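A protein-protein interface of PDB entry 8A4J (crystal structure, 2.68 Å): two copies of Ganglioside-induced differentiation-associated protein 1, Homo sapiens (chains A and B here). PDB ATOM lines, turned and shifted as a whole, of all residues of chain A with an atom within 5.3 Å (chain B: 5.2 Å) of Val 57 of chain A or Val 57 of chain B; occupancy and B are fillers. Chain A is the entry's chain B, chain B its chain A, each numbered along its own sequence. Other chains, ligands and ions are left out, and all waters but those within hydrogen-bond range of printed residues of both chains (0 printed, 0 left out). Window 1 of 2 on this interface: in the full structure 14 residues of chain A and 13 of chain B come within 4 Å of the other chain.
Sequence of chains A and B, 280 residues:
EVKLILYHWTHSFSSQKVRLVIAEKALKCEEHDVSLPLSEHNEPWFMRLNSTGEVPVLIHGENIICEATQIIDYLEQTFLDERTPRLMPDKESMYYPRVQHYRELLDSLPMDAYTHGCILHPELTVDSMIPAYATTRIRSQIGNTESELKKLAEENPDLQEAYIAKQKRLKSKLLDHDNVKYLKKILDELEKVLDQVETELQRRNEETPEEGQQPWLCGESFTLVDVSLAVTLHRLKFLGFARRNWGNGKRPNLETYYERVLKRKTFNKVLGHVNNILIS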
ATOM      1  N   ILE A   5      -7.974   3.973  -1.291  1.00  0.00           N
ATOM      2  CA  ILE A   5      -6.791   4.624  -0.712  1.00  0.00           C
ATOM      3  C   ILE A   5      -5.582   3.696  -0.669  1.00  0.00           C
ATOM      4  O   ILE A   5      -5.688   2.527  -0.286  1.00  0.00           O
ATOM      5  CB  ILE A   5      -7.078   5.168   0.694  1.00  0.00           C
ATOM      6  CG1 ILE A   5      -8.303   6.076   0.664  1.00  0.00           C
ATOM      7  CG2 ILE A   5      -5.861   5.891   1.181  1.00  0.00           C
ATOM      8  CD1 ILE A   5      -8.738   6.576   1.988  1.00  0.00           C
ATOM      9  N   LEU A   6      -4.414   4.237  -1.029  1.00  0.00           N
ATOM     10  CA  LEU A   6      -3.200   3.434  -1.168  1.00  0.00           C
ATOM     11  C   LEU A   6      -2.049   4.141  -0.467  1.00  0.00           C
ATOM     12  O   LEU A   6      -1.737   5.303  -0.765  1.00  0.00           O
ATOM     13  CB  LEU A   6      -2.844   3.188  -2.643  1.00  0.00           C
ATOM     14  CG  LEU A   6      -1.568   2.369  -2.864  1.00  0.00           C
ATOM     15  CD1 LEU A   6      -1.720   0.871  -2.605  1.00  0.00           C
ATOM     16  CD2 LEU A   6      -1.059   2.561  -4.243  1.00  0.00           C
ATOM     17  N   TYR A   7      -1.429   3.449   0.471  1.00  0.00           N
ATOM     18  CA  TYR A   7      -0.263   3.960   1.174  1.00  0.00           C
ATOM     19  C   TYR A   7       0.921   3.106   0.723  1.00  0.00           C
ATOM     20  O   TYR A   7       0.872   1.864   0.821  1.00  0.00           O
ATOM     21  CB  TYR A   7      -0.487   3.955   2.705  1.00  0.00           C
ATOM     22  CG  TYR A   7      -1.388   5.071   3.248  1.00  0.00           C
ATOM     23  CD1 TYR A   7      -0.881   6.347   3.521  1.00  0.00           C
ATOM     24  CD2 TYR A   7      -2.718   4.833   3.535  1.00  0.00           C
ATOM     25  CE1 TYR A   7      -1.679   7.353   4.024  1.00  0.00           C
ATOM     26  CE2 TYR A   7      -3.545   5.843   4.074  1.00  0.00           C
ATOM     27  CZ  TYR A   7      -3.018   7.088   4.302  1.00  0.00           C
ATOM     28  OH  TYR A   7      -3.834   8.068   4.825  1.00  0.00           O
ATOM     29  N   HIS A   8       1.968   3.772   0.213  1.00  0.00           N
ATOM     30  CA  HIS A   8       2.999   3.093  -0.560  1.00  0.00           C
ATOM     31  C   HIS A   8       4.259   3.944  -0.530  1.00  0.00           C
ATOM     32  O   HIS A   8       4.225   5.120  -0.145  1.00  0.00           O
ATOM     33  CB  HIS A   8       2.524   2.875  -2.015  1.00  0.00           C
ATOM     34  CG  HIS A   8       2.527   4.129  -2.844  1.00  0.00           C
ATOM     35  ND1 HIS A   8       1.564   5.108  -2.732  1.00  0.00           N
ATOM     36  CD2 HIS A   8       3.408   4.586  -3.759  1.00  0.00           C
ATOM     37  CE1 HIS A   8       1.846   6.110  -3.549  1.00  0.00           C
ATOM     38  NE2 HIS A   8       2.957   5.813  -4.189  1.00  0.00           N
ATOM     39  N   VAL A  55       6.034  -2.898   2.864  1.00  0.00           N
ATOM     40  CA  VAL A  55       4.750  -3.463   2.404  1.00  0.00           C
ATOM     41  C   VAL A  55       3.607  -2.444   2.225  1.00  0.00           C
ATOM     42  O   VAL A  55       3.248  -1.773   3.168  1.00  0.00           O
ATOM     43  CB  VAL A  55       4.317  -4.518   3.387  1.00  0.00           C
ATOM     44  CG1 VAL A  55       4.087  -3.782   4.774  1.00  0.00           C
ATOM     45  CG2 VAL A  55       3.130  -5.214   2.870  1.00  0.00           C
ATOM     46  N   PRO A  56       3.053  -2.301   1.031  1.00  0.00           N
ATOM     47  CA  PRO A  56       2.006  -1.280   0.834  1.00  0.00           C
ATOM     48  C   PRO A  56       0.648  -1.724   1.385  1.00  0.00           C
ATOM     49  O   PRO A  56       0.427  -2.913   1.653  1.00  0.00           O
ATOM     50  CB  PRO A  56       1.947  -1.127  -0.702  1.00  0.00           C
ATOM     51  CG  PRO A  56       2.346  -2.465  -1.225  1.00  0.00           C
ATOM     52  CD  PRO A  56       3.313  -3.087  -0.195  1.00  0.00           C
ATOM     53  N   VAL A  57      -0.277  -0.758   1.533  1.00  0.00           N
ATOM     54  CA  VAL A  57      -1.611  -1.067   2.058  1.00  0.00           C
ATOM     55  C   VAL A  57      -2.716  -0.346   1.305  1.00  0.00           C
ATOM     56  O   VAL A  57      -2.556   0.808   0.896  1.00  0.00           O
ATOM     57  CB  VAL A  57      -1.721  -0.723   3.549  1.00  0.00           C
ATOM     58  CG1 VAL A  57      -1.658   0.789   3.736  1.00  0.00           C
ATOM     59  CG2 VAL A  57      -3.031  -1.194   4.097  1.00  0.00           C
ATOM     60  N   LEU A  58      -3.825  -1.059   1.084  1.00  0.00           N
ATOM     61  CA  LEU A  58      -5.004  -0.526   0.416  1.00  0.00           C
ATOM     62  C   LEU A  58      -6.216  -0.519   1.363  1.00  0.00           C
ATOM     63  O   LEU A  58      -6.551  -1.529   2.019  1.00  0.00           O
ATOM     64  CB  LEU A  58      -5.335  -1.311  -0.864  1.00  0.00           C
ATOM     65  CG  LEU A  58      -6.566  -0.791  -1.613  1.00  0.00           C
ATOM     66  CD1 LEU A  58      -6.219   0.350  -2.486  1.00  0.00           C
ATOM     67  CD2 LEU A  58      -7.295  -1.868  -2.400  1.00  0.00           C
ATOM     68  N   ILE A  59      -6.898   0.613   1.384  1.00  0.00           N
ATOM     69  CA  ILE A  59      -8.087   0.804   2.171  1.00  0.00           C
ATOM     70  C   ILE A  59      -9.183   1.139   1.193  1.00  0.00           C
ATOM     71  O   ILE A  59      -9.083   2.128   0.467  1.00  0.00           O
ATOM     72  CB  ILE A  59      -7.904   1.912   3.222  1.00  0.00           C
ATOM     73  CG1 ILE A  59      -6.803   1.518   4.200  1.00  0.00           C
ATOM     74  CG2 ILE A  59      -9.186   2.126   3.996  1.00  0.00           C
ATOM     75  CD1 ILE A  59      -5.611   2.357   4.126  1.00  0.00           C
ATOM     76  N   ILE A  64      -9.154  -3.595   4.479  1.00  0.00           N
ATOM     77  CA  ILE A  64      -7.754  -3.227   4.574  1.00  0.00           C
ATOM     78  C   ILE A  64      -6.943  -4.376   4.003  1.00  0.00           C
ATOM     79  O   ILE A  64      -6.959  -5.483   4.556  1.00  0.00           O
ATOM     80  CB  ILE A  64      -7.357  -2.968   6.034  1.00  0.00           C
ATOM     81  CG1 ILE A  64      -8.039  -1.702   6.544  1.00  0.00           C
ATOM     82  CG2 ILE A  64      -5.851  -2.792   6.191  1.00  0.00           C
ATOM     83  CD1 ILE A  64      -8.400  -1.768   8.037  1.00  0.00           C
ATOM     84  N   ILE A  65      -6.148  -4.097   2.986  1.00  0.00           N
ATOM     85  CA  ILE A  65      -5.338  -5.139   2.374  1.00  0.00           C
ATOM     86  C   ILE A  65      -3.873  -4.721   2.330  1.00  0.00           C
ATOM     87  O   ILE A  65      -3.548  -3.570   2.013  1.00  0.00           O
ATOM     88  CB  ILE A  65      -5.864  -5.490   0.962  1.00  0.00           C
ATOM     89  CG1 ILE A  65      -7.386  -5.749   0.984  1.00  0.00           C
ATOM     90  CG2 ILE A  65      -5.225  -6.770   0.462  1.00  0.00           C
ATOM     91  CD1 ILE A  65      -8.226  -4.502   0.695  1.00  0.00           C
ATOM     92  N   CYS A  66      -3.004  -5.685   2.648  1.00  0.00           N
ATOM     93  CA  CYS A  66      -1.566  -5.501   2.774  1.00  0.00           C
ATOM     94  C   CYS A  66      -0.790  -6.501   1.910  1.00  0.00           C
ATOM     95  O   CYS A  66      -1.218  -7.664   1.775  1.00  0.00           O
ATOM     96  CB  CYS A  66      -1.169  -5.661   4.262  1.00  0.00           C
ATOM     97  SG  CYS A  66      -1.897  -4.428   5.418  1.00  0.00           S
ATOM     98  N   ILE A  71      -3.109  -7.030  -2.585  1.00  0.00           N
ATOM     99  CA  ILE A  71      -3.852  -5.869  -3.041  1.00  0.00           C
ATOM    100  C   ILE A  71      -4.308  -6.087  -4.467  1.00  0.00           C
ATOM    101  O   ILE A  71      -5.379  -5.625  -4.861  1.00  0.00           O
ATOM    102  CB  ILE A  71      -2.992  -4.596  -2.923  1.00  0.00           C
ATOM    103  CG1 ILE A  71      -2.714  -4.306  -1.441  1.00  0.00           C
ATOM    104  CG2 ILE A  71      -3.724  -3.437  -3.629  1.00  0.00           C
ATOM    105  CD1 ILE A  71      -1.618  -3.163  -1.162  1.00  0.00           C
ATOM    106  N   ILE B   5      -1.403   7.408  12.119  1.00  0.00           N
ATOM    107  CA  ILE B   5      -2.692   7.158  11.488  1.00  0.00           C
ATOM    108  C   ILE B   5      -3.031   5.695  11.620  1.00  0.00           C
ATOM    109  O   ILE B   5      -2.186   4.833  11.377  1.00  0.00           O
ATOM    110  CB  ILE B   5      -2.702   7.602  10.024  1.00  0.00           C
ATOM    111  CG1 ILE B   5      -2.206   9.045   9.968  1.00  0.00           C
ATOM    112  CG2 ILE B   5      -4.091   7.492   9.513  1.00  0.00           C
ATOM    113  CD1 ILE B   5      -2.098   9.589   8.577  1.00  0.00           C
ATOM    114  N   LEU B   6      -4.252   5.413  12.027  1.00  0.00           N
ATOM    115  CA  LEU B   6      -4.648   4.047  12.301  1.00  0.00           C
ATOM    116  C   LEU B   6      -5.981   3.769  11.629  1.00  0.00           C
ATOM    117  O   LEU B   6      -6.983   4.457  11.877  1.00  0.00           O
ATOM    118  CB  LEU B   6      -4.758   3.755  13.802  1.00  0.00           C
ATOM    119  CG  LEU B   6      -5.249   2.320  14.042  1.00  0.00           C
ATOM    120  CD1 LEU B   6      -4.194   1.288  13.780  1.00  0.00           C
ATOM    121  CD2 LEU B   6      -5.758   2.117  15.465  1.00  0.00           C
ATOM    122  N   TYR B   7      -5.974   2.736  10.805  1.00  0.00           N
ATOM    123  CA  TYR B   7      -7.133   2.221  10.116  1.00  0.00           C
ATOM    124  C   TYR B   7      -7.420   0.873  10.751  1.00  0.00           C
ATOM    125  O   TYR B   7      -6.517   0.020  10.831  1.00  0.00           O
ATOM    126  CB  TYR B   7      -6.822   2.098   8.634  1.00  0.00           C
ATOM    127  CG  TYR B   7      -6.689   3.434   7.899  1.00  0.00           C
ATOM    128  CD1 TYR B   7      -7.795   4.102   7.433  1.00  0.00           C
ATOM    129  CD2 TYR B   7      -5.446   3.972   7.606  1.00  0.00           C
ATOM    130  CE1 TYR B   7      -7.684   5.283   6.756  1.00  0.00           C
ATOM    131  CE2 TYR B   7      -5.327   5.155   6.910  1.00  0.00           C
ATOM    132  CZ  TYR B   7      -6.464   5.821   6.503  1.00  0.00           C
ATOM    133  OH  TYR B   7      -6.406   7.014   5.789  1.00  0.00           O
ATOM    134  N   VAL B  55      -7.367  -7.135  10.134  1.00  0.00           N
ATOM    135  CA  VAL B  55      -5.952  -6.863  10.319  1.00  0.00           C
ATOM    136  C   VAL B  55      -5.804  -5.348  10.136  1.00  0.00           C
ATOM    137  O   VAL B  55      -6.002  -4.819   9.031  1.00  0.00           O
ATOM    138  CB  VAL B  55      -5.101  -7.727   9.366  1.00  0.00           C
ATOM    139  CG1 VAL B  55      -5.809  -7.884   8.071  1.00  0.00           C
ATOM    140  CG2 VAL B  55      -3.754  -7.069   9.154  1.00  0.00           C
ATOM    141  N   PRO B  56      -5.485  -4.610  11.202  1.00  0.00           N
ATOM    142  CA  PRO B  56      -5.373  -3.152  11.094  1.00  0.00           C
ATOM    143  C   PRO B  56      -4.001  -2.716  10.589  1.00  0.00           C
ATOM    144  O   PRO B  56      -3.052  -3.501  10.499  1.00  0.00           O
ATOM    145  CB  PRO B  56      -5.594  -2.664  12.499  1.00  0.00           C
ATOM    146  CG  PRO B  56      -5.030  -3.825  13.347  1.00  0.00           C
ATOM    147  CD  PRO B  56      -5.203  -5.089  12.572  1.00  0.00           C
ATOM    148  N   VAL B  57      -3.915  -1.451  10.234  1.00  0.00           N
ATOM    149  CA  VAL B  57      -2.677  -0.936   9.698  1.00  0.00           C
ATOM    150  C   VAL B  57      -2.363   0.417  10.327  1.00  0.00           C
ATOM    151  O   VAL B  57      -3.257   1.253  10.529  1.00  0.00           O
ATOM    152  CB  VAL B  57      -2.736  -0.823   8.167  1.00  0.00           C
ATOM    153  CG1 VAL B  57      -3.640   0.289   7.764  1.00  0.00           C
ATOM    154  CG2 VAL B  57      -1.339  -0.588   7.609  1.00  0.00           C
ATOM    155  N   LEU B  58      -1.084   0.610  10.648  1.00  0.00           N
ATOM    156  CA  LEU B  58      -0.578   1.854  11.208  1.00  0.00           C
ATOM    157  C   LEU B  58       0.350   2.521  10.202  1.00  0.00           C
ATOM    158  O   LEU B  58       1.177   1.853   9.551  1.00  0.00           O
ATOM    159  CB  LEU B  58       0.153   1.613  12.521  1.00  0.00           C
ATOM    160  CG  LEU B  58       0.711   2.862  13.135  1.00  0.00           C
ATOM    161  CD1 LEU B  58      -0.359   3.656  13.831  1.00  0.00           C
ATOM    162  CD2 LEU B  58       1.815   2.497  14.144  1.00  0.00           C
ATOM    163  N   ILE B  59       0.144   3.821  10.010  1.00  0.00           N
ATOM    164  CA  ILE B  59       0.991   4.617   9.150  1.00  0.00           C
ATOM    165  C   ILE B  59       1.604   5.677  10.036  1.00  0.00           C
ATOM    166  O   ILE B  59       0.898   6.531  10.594  1.00  0.00           O
ATOM    167  CB  ILE B  59       0.231   5.267   7.988  1.00  0.00           C
ATOM    168  CG1 ILE B  59      -0.417   4.204   7.135  1.00  0.00           C
ATOM    169  CG2 ILE B  59       1.215   6.083   7.113  1.00  0.00           C
ATOM    170  CD1 ILE B  59      -1.823   4.316   7.127  1.00  0.00           C
ATOM    171  N   ILE B  64       4.686   1.830   7.178  1.00  0.00           N
ATOM    172  CA  ILE B  64       3.393   1.187   7.106  1.00  0.00           C
ATOM    173  C   ILE B  64       3.534  -0.125   7.866  1.00  0.00           C
ATOM    174  O   ILE B  64       4.404  -0.944   7.553  1.00  0.00           O
ATOM    175  CB  ILE B  64       2.970   0.965   5.650  1.00  0.00           C
ATOM    176  CG1 ILE B  64       2.573   2.312   5.039  1.00  0.00           C
ATOM    177  CG2 ILE B  64       1.791   0.061   5.541  1.00  0.00           C
ATOM    178  CD1 ILE B  64       2.920   2.441   3.596  1.00  0.00           C
ATOM    179  N   ILE B  65       2.731  -0.299   8.901  1.00  0.00           N
ATOM    180  CA  ILE B  65       2.777  -1.527   9.675  1.00  0.00           C
ATOM    181  C   ILE B  65       1.380  -2.091   9.799  1.00  0.00           C
ATOM    182  O   ILE B  65       0.437  -1.382  10.177  1.00  0.00           O
ATOM    183  CB  ILE B  65       3.399  -1.314  11.062  1.00  0.00           C
ATOM    184  CG1 ILE B  65       4.714  -0.578  10.914  1.00  0.00           C
ATOM    185  CG2 ILE B  65       3.728  -2.621  11.740  1.00  0.00           C
ATOM    186  CD1 ILE B  65       4.515   0.910  11.032  1.00  0.00           C
ATOM    187  N   CYS B  66       1.275  -3.390   9.570  1.00  0.00           N
ATOM    188  CA  CYS B  66       0.012  -4.111   9.467  1.00  0.00           C
ATOM    189  C   CYS B  66       0.059  -5.229  10.501  1.00  0.00           C
ATOM    190  O   CYS B  66       1.143  -5.791  10.744  1.00  0.00           O
ATOM    191  CB  CYS B  66      -0.197  -4.748   8.055  1.00  0.00           C
ATOM    192  SG  CYS B  66      -0.274  -3.686   6.551  1.00  0.00           S
ATOM    193  N   GLU B  67      -1.119  -5.552  11.079  1.00  0.00           N
ATOM    194  CA  GLU B  67      -1.322  -6.604  12.086  1.00  0.00           C
ATOM    195  C   GLU B  67      -0.968  -6.126  13.485  1.00  0.00           C
ATOM    196  O   GLU B  67       0.021  -5.420  13.670  1.00  0.00           O
ATOM    197  CB  GLU B  67      -0.561  -7.884  11.787  1.00  0.00           C
ATOM    198  CG  GLU B  67      -1.043  -8.629  10.470  1.00  0.00           C
ATOM    199  CD  GLU B  67      -0.141  -9.822  10.091  1.00  0.00           C
ATOM    200  OE1 GLU B  67       0.892 -10.050  10.775  1.00  0.00           O
ATOM    201  OE2 GLU B  67      -0.428 -10.531   9.084  1.00  0.00           O
ATOM    202  N   ILE B  71       2.128  -3.918  14.988  1.00  0.00           N
ATOM    203  CA  ILE B  71       1.932  -2.521  15.328  1.00  0.00           C
ATOM    204  C   ILE B  71       2.337  -2.275  16.782  1.00  0.00           C
ATOM    205  O   ILE B  71       2.996  -1.277  17.126  1.00  0.00           O
ATOM    206  CB  ILE B  71       0.456  -2.156  15.125  1.00  0.00           C
ATOM    207  CG1 ILE B  71       0.079  -2.176  13.658  1.00  0.00           C
ATOM    208  CG2 ILE B  71       0.177  -0.833  15.739  1.00  0.00           C
ATOM    209  CD1 ILE B  71      -1.421  -2.050  13.472  1.00  0.00           C
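SG of Cys 66 of chain B is disulfide-bonded to SG of Cys 66 of chain A (2.1 Å).
OH of Tyr 7 of chain A lies within hydrogen-bond range of OH of Tyr 7 of chain B (2.9 Å).
N of Tyr 7 of chain A lies within hydrogen-bond range of O of Val 57 of chain A.
O of Ile 5 of chain B lies within hydrogen-bond range of N of Ile 59 of chain B.
The backbone carbonyl oxygen of Ile 59 of chain A lies within hydrogen-bond range of the backbone NH of Ile 5 of chain A, at 2.8 Å.
O of Tyr 7 of chain B lies within hydrogen-bond range of N of Val 57 of chain B.
Among the printed residues, pairs that only touch across the chains: Val 55 of chain A with Ile 64 of chain B (3.3 Å), Ile 64 of chain A with Val 55 of chain B (3.5 Å), Tyr 7 of chain A with Ile 64 of chain B (3.5 Å), Tyr 7 of chain A with Ile 59 of chain B (3.7 Å), His 8 of chain A with Ile 64 of chain B (3.8 Å), Ile 64 of chain A with Tyr 7 of chain B (3.8 Å), Ile 59 of chain A with Tyr 7 of chain B (3.8 Å), Val 57 of chain A with Val 57 of chain B (3.9 Å) and Val 57 of chain A with Ile 64 of chain B (3.96 Å).
Of the printed residues of chain B, Val 57 of chain A touches Val 57 (3.9 Å) and Ile 64 (3.96 Å).
Of the printed residues of chain A, Val 57 of chain B touches Val 57.
Of the printed residues of chain B, His 8 of chain A touches Ile 64 (3.8 Å).
Of the printed residues of chain B, Ile 59 of chain A touches Tyr 7 (3.8 Å).
Printed residues of chain A within 4 Å of Cys 66 of chain B: Cys 66 (2.1 Å).
Leu 58 of chain B touches none of the printed residues of chain A.
Hydrophobic or aromatic side chains of chain A that line the printed part of chain B: Tyr 7, Val 55, Val 57, Ile 59 and Ile 64.
Along chain A the printed residues that touch a printed residue of chain B span positions 7 to 66.
Tyr 7 of chain A touches Ile 59 of chain B, and with the chains exchanged Ile 59 of chain A touches Tyr 7 of chain B.
Val 55 of chain A touches Ile 64 of chain B, and with the chains exchanged Ile 64 of chain A touches Val 55 of chain B.
Val 57 of chain A touches Ile 64 of chain B, but with the chains exchanged Ile 64 of chain A does not touch Val 57 of chain B (4.1 Å).
Cys 66 of chain A touches its own counterpart, Cys 66 of chain B.
Of the 11 pairs that touch across the chains among the printed residues, 9 have their exchanged pair printed and touching as well.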
